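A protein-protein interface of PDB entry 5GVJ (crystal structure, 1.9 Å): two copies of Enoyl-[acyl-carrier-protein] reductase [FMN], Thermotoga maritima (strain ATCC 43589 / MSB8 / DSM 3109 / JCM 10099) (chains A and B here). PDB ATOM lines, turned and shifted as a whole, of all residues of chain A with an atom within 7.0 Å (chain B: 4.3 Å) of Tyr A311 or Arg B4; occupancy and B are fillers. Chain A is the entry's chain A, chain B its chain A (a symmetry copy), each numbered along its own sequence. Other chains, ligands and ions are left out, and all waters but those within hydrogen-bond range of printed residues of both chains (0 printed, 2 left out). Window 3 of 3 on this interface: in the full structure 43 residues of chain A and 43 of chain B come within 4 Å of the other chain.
The side-chain carboxylate (OD1) of Asp B9 lies within salt-bridge range of the guanidinium group (NE) of Arg B4, at 2.9 Å. The side-chain hydroxyl of Tyr A311 is in hydrogen-bond range of the side-chain amino group of Lys A307 (2.8 Å). OG1 of Thr B5 sits at hydrogen-bond distance from O of Glu B188. The side-chain hydroxyl (OG1) of Thr B8 sits at hydrogen-bond distance from the backbone carbonyl oxygen (O) of Thr B5.
Among the printed residues, pairs that only touch across the chains: Leu A308 with Phe B183, Tyr A311 with Arg B4, Tyr A311 with Thr B5, Tyr A311 with Phe B183 and Ile A312 with Phe B301.
Of chain B, only Arg B4, Thr B5 and Phe B183 come within 4 Å of Tyr A311. Of the printed residues of chain B, Ile A312 touches Phe B301. Printed residues of chain A within 4 Å of Phe B301: Ile A312 (3.9 Å). Of the printed residues of chain A, Thr B5 touches Tyr A311. Thr B8 touches none of the printed residues of chain A. Asp B9 touches none of the printed residues of chain A. The nearest printed residue of chain B that does not touch Tyr A311 is Phe B301 (4.1 Å).
Along chain A the printed residues that touch a printed residue of chain B span positions 308 to 312. Hydrophobic or aromatic side chains of chain B that line the printed part of chain A: Phe B183 and Phe B301. Among the printed residues, no Asp or Glu carboxylate lies within 4 Å of a Lys or Arg side-chain nitrogen of the other chain.
No position is printed for both chains. Of the 5 pairs that touch across the chains among the printed residues, none has its exchanged pair printed and touching as well.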
ATOM      1  N   GLU A 306      29.267  19.647  26.113  1.00  0.00           N
ATOM      2  CA  GLU A 306      30.221  20.621  26.637  1.00  0.00           C
ATOM      3  C   GLU A 306      30.099  21.955  25.921  1.00  0.00           C
ATOM      4  O   GLU A 306      30.167  23.016  26.553  1.00  0.00           O
ATOM      5  CB  GLU A 306      31.648  20.084  26.516  1.00  0.00           C
ATOM      6  CG  GLU A 306      31.832  18.799  27.288  1.00  0.00           C
ATOM      7  CD  GLU A 306      33.214  18.216  27.146  1.00  0.00           C
ATOM      8  OE1 GLU A 306      33.663  17.562  28.110  1.00  0.00           O
ATOM      9  OE2 GLU A 306      33.843  18.400  26.080  1.00  0.00           O
ATOM     10  N   LYS A 307      29.914  21.925  24.600  1.00  0.00           N
ATOM     11  CA  LYS A 307      29.722  23.159  23.843  1.00  0.00           C
ATOM     12  C   LYS A 307      28.476  23.904  24.315  1.00  0.00           C
ATOM     13  O   LYS A 307      28.519  25.117  24.558  1.00  0.00           O
ATOM     14  CB  LYS A 307      29.634  22.838  22.349  1.00  0.00           C
ATOM     15  CG  LYS A 307      29.914  24.011  21.406  1.00  0.00           C
ATOM     16  CD  LYS A 307      28.895  24.079  20.269  1.00  0.00           C
ATOM     17  CE  LYS A 307      29.203  25.248  19.331  1.00  0.00           C
ATOM     18  NZ  LYS A 307      28.120  26.298  19.341  1.00  0.00           N
ATOM     19  N   LEU A 308      27.355  23.190  24.460  1.00  0.00           N
ATOM     20  CA  LEU A 308      26.127  23.830  24.937  1.00  0.00           C
ATOM     21  C   LEU A 308      26.311  24.409  26.331  1.00  0.00           C
ATOM     22  O   LEU A 308      25.767  25.475  26.650  1.00  0.00           O
ATOM     23  CB  LEU A 308      24.972  22.831  24.943  1.00  0.00           C
ATOM     24  CG  LEU A 308      24.521  22.322  23.575  1.00  0.00           C
ATOM     25  CD1 LEU A 308      23.408  21.296  23.723  1.00  0.00           C
ATOM     26  CD2 LEU A 308      24.051  23.477  22.743  1.00  0.00           C
ATOM     27  N   ARG A 309      27.057  23.704  27.184  1.00  0.00           N
ATOM     28  CA  ARG A 309      27.292  24.177  28.542  1.00  0.00           C
ATOM     29  C   ARG A 309      27.989  25.527  28.539  1.00  0.00           C
ATOM     30  O   ARG A 309      27.785  26.336  29.454  1.00  0.00           O
ATOM     31  CB  ARG A 309      28.103  23.129  29.307  1.00  0.00           C
ATOM     32  CG  ARG A 309      28.806  23.625  30.548  1.00  0.00           C
ATOM     33  CD  ARG A 309      29.903  22.647  30.936  1.00  0.00           C
ATOM     34  NE  ARG A 309      29.366  21.416  31.505  1.00  0.00           N
ATOM     35  CZ  ARG A 309      30.064  20.294  31.632  1.00  0.00           C
ATOM     36  NH1 ARG A 309      31.320  20.250  31.206  1.00  0.00           N
ATOM     37  NH2 ARG A 309      29.503  19.219  32.172  1.00  0.00           N
ATOM     38  N   GLY A 310      28.773  25.807  27.498  1.00  0.00           N
ATOM     39  CA  GLY A 310      29.445  27.088  27.409  1.00  0.00           C
ATOM     40  C   GLY A 310      28.488  28.262  27.420  1.00  0.00           C
ATOM     41  O   GLY A 310      28.852  29.355  27.856  1.00  0.00           O
ATOM     42  N   TYR A 311      27.251  28.056  26.958  1.00  0.00           N
ATOM     43  CA  TYR A 311      26.284  29.145  26.888  1.00  0.00           C
ATOM     44  C   TYR A 311      25.656  29.481  28.237  1.00  0.00           C
ATOM     45  O   TYR A 311      25.239  30.625  28.435  1.00  0.00           O
ATOM     46  CB  TYR A 311      25.186  28.812  25.863  1.00  0.00           C
ATOM     47  CG  TYR A 311      25.701  28.752  24.440  1.00  0.00           C
ATOM     48  CD1 TYR A 311      26.173  29.888  23.808  1.00  0.00           C
ATOM     49  CD2 TYR A 311      25.728  27.550  23.735  1.00  0.00           C
ATOM     50  CE1 TYR A 311      26.649  29.836  22.509  1.00  0.00           C
ATOM     51  CE2 TYR A 311      26.204  27.486  22.440  1.00  0.00           C
ATOM     52  CZ  TYR A 311      26.665  28.633  21.834  1.00  0.00           C
ATOM     53  OH  TYR A 311      27.147  28.578  20.546  1.00  0.00           O
ATOM     54  N   ILE A 312      25.590  28.533  29.170  1.00  0.00           N
ATOM     55  CA  ILE A 312      24.871  28.759  30.429  1.00  0.00           C
ATOM     56  C   ILE A 312      25.816  28.912  31.623  1.00  0.00           C
ATOM     57  O   ILE A 312      26.970  28.468  31.585  1.00  0.00           O
ATOM     58  CB  ILE A 312      23.866  27.628  30.705  1.00  0.00           C
ATOM     59  CG1 ILE A 312      24.614  26.332  31.042  1.00  0.00           C
ATOM     60  CG2 ILE A 312      22.926  27.442  29.511  1.00  0.00           C
ATOM     61  CD1 ILE A 312      23.794  25.318  31.839  1.00  0.00           C
ATOM     62  N   VAL B   3      21.832  34.286  26.956  1.00  0.00           N
ATOM     63  CA  VAL B   3      22.906  33.518  26.348  1.00  0.00           C
ATOM     64  C   VAL B   3      23.511  34.363  25.236  1.00  0.00           C
ATOM     65  O   VAL B   3      22.805  35.115  24.557  1.00  0.00           O
ATOM     66  CB  VAL B   3      22.407  32.145  25.839  1.00  0.00           C
ATOM     67  CG1 VAL B   3      21.159  31.717  26.602  1.00  0.00           C
ATOM     68  CG2 VAL B   3      22.175  32.120  24.336  1.00  0.00           C
ATOM     69  N   ARG B   4      24.824  34.284  25.096  1.00  0.00           N
ATOM     70  CA  ARG B   4      25.558  35.061  24.111  1.00  0.00           C
ATOM     71  C   ARG B   4      26.055  34.122  23.022  1.00  0.00           C
ATOM     72  O   ARG B   4      26.541  33.033  23.321  1.00  0.00           O
ATOM     73  CB  ARG B   4      26.729  35.784  24.777  1.00  0.00           C
ATOM     74  CG  ARG B   4      27.446  36.763  23.884  1.00  0.00           C
ATOM     75  CD  ARG B   4      28.573  37.466  24.636  1.00  0.00           C
ATOM     76  NE  ARG B   4      29.303  38.374  23.755  1.00  0.00           N
ATOM     77  CZ  ARG B   4      30.156  39.300  24.176  1.00  0.00           C
ATOM     78  NH1 ARG B   4      30.398  39.439  25.475  1.00  0.00           N
ATOM     79  NH2 ARG B   4      30.758  40.089  23.299  1.00  0.00           N
ATOM     80  N   THR B   5      25.893  34.512  21.758  1.00  0.00           N
ATOM     81  CA  THR B   5      26.385  33.698  20.647  1.00  0.00           C
ATOM     82  C   THR B   5      27.024  34.609  19.612  1.00  0.00           C
ATOM     83  O   THR B   5      26.913  35.834  19.684  1.00  0.00           O
ATOM     84  CB  THR B   5      25.281  32.879  19.972  1.00  0.00           C
ATOM     85  OG1 THR B   5      24.530  33.719  19.088  1.00  0.00           O
ATOM     86  CG2 THR B   5      24.316  32.260  21.008  1.00  0.00           C
ATOM     87  N   THR B   8      24.256  37.005  18.387  1.00  0.00           N
ATOM     88  CA  THR B   8      23.946  38.214  19.151  1.00  0.00           C
ATOM     89  C   THR B   8      25.072  39.241  19.033  1.00  0.00           C
ATOM     90  O   THR B   8      24.814  40.452  19.031  1.00  0.00           O
ATOM     91  CB  THR B   8      23.661  37.880  20.621  1.00  0.00           C
ATOM     92  OG1 THR B   8      24.833  37.353  21.256  1.00  0.00           O
ATOM     93  CG2 THR B   8      22.539  36.873  20.725  1.00  0.00           C
ATOM     94  N   ASP B   9      26.318  38.780  18.896  1.00  0.00           N
ATOM     95  CA  ASP B   9      27.424  39.703  18.664  1.00  0.00           C
ATOM     96  C   ASP B   9      27.326  40.337  17.286  1.00  0.00           C
ATOM     97  O   ASP B   9      27.447  41.559  17.144  1.00  0.00           O
ATOM     98  CB  ASP B   9      28.757  38.976  18.815  1.00  0.00           C
ATOM     99  CG  ASP B   9      29.056  38.619  20.244  1.00  0.00           C
ATOM    100  OD1 ASP B   9      28.665  39.401  21.134  1.00  0.00           O
ATOM    101  OD2 ASP B   9      29.689  37.565  20.469  1.00  0.00           O
ATOM    102  N   PHE B 183      20.931  24.437  18.594  1.00  0.00           N
ATOM    103  CA  PHE B 183      22.317  24.739  18.936  1.00  0.00           C
ATOM    104  C   PHE B 183      23.172  23.477  18.925  1.00  0.00           C
ATOM    105  O   PHE B 183      24.338  23.502  18.501  1.00  0.00           O
ATOM    106  CB  PHE B 183      22.356  25.428  20.305  1.00  0.00           C
ATOM    107  CG  PHE B 183      22.050  26.907  20.252  1.00  0.00           C
ATOM    108  CD1 PHE B 183      21.102  27.407  19.371  1.00  0.00           C
ATOM    109  CD2 PHE B 183      22.714  27.791  21.085  1.00  0.00           C
ATOM    110  CE1 PHE B 183      20.827  28.769  19.315  1.00  0.00           C
ATOM    111  CE2 PHE B 183      22.435  29.153  21.042  1.00  0.00           C
ATOM    112  CZ  PHE B 183      21.492  29.634  20.156  1.00  0.00           C
ATOM    113  N   GLU B 188      23.638  28.885  15.906  1.00  0.00           N
ATOM    114  CA  GLU B 188      23.930  29.848  16.960  1.00  0.00           C
ATOM    115  C   GLU B 188      22.810  30.870  17.142  1.00  0.00           C
ATOM    116  O   GLU B 188      22.984  31.839  17.886  1.00  0.00           O
ATOM    117  CB  GLU B 188      25.274  30.524  16.678  1.00  0.00           C
ATOM    118  CG  GLU B 188      26.356  29.451  16.597  1.00  0.00           C
ATOM    119  CD  GLU B 188      27.718  29.980  16.219  1.00  0.00           C
ATOM    120  OE1 GLU B 188      28.381  30.551  17.099  1.00  0.00           O
ATOM    121  OE2 GLU B 188      28.123  29.805  15.055  1.00  0.00           O
ATOM    122  N   PHE B 301      15.618  26.742  27.598  1.00  0.00           N
ATOM    123  CA  PHE B 301      16.914  26.458  26.986  1.00  0.00           C
ATOM    124  C   PHE B 301      17.938  26.097  28.056  1.00  0.00           C
ATOM    125  O   PHE B 301      18.624  25.072  27.959  1.00  0.00           O
ATOM    126  CB  PHE B 301      17.381  27.667  26.169  1.00  0.00           C
ATOM    127  CG  PHE B 301      18.816  27.574  25.717  1.00  0.00           C
ATOM    128  CD1 PHE B 301      19.144  26.938  24.530  1.00  0.00           C
ATOM    129  CD2 PHE B 301      19.838  28.115  26.486  1.00  0.00           C
ATOM    130  CE1 PHE B 301      20.471  26.854  24.110  1.00  0.00           C
ATOM    131  CE2 PHE B 301      21.152  28.029  26.078  1.00  0.00           C
ATOM    132  CZ  PHE B 301      21.469  27.390  24.894  1.00  0.00           C
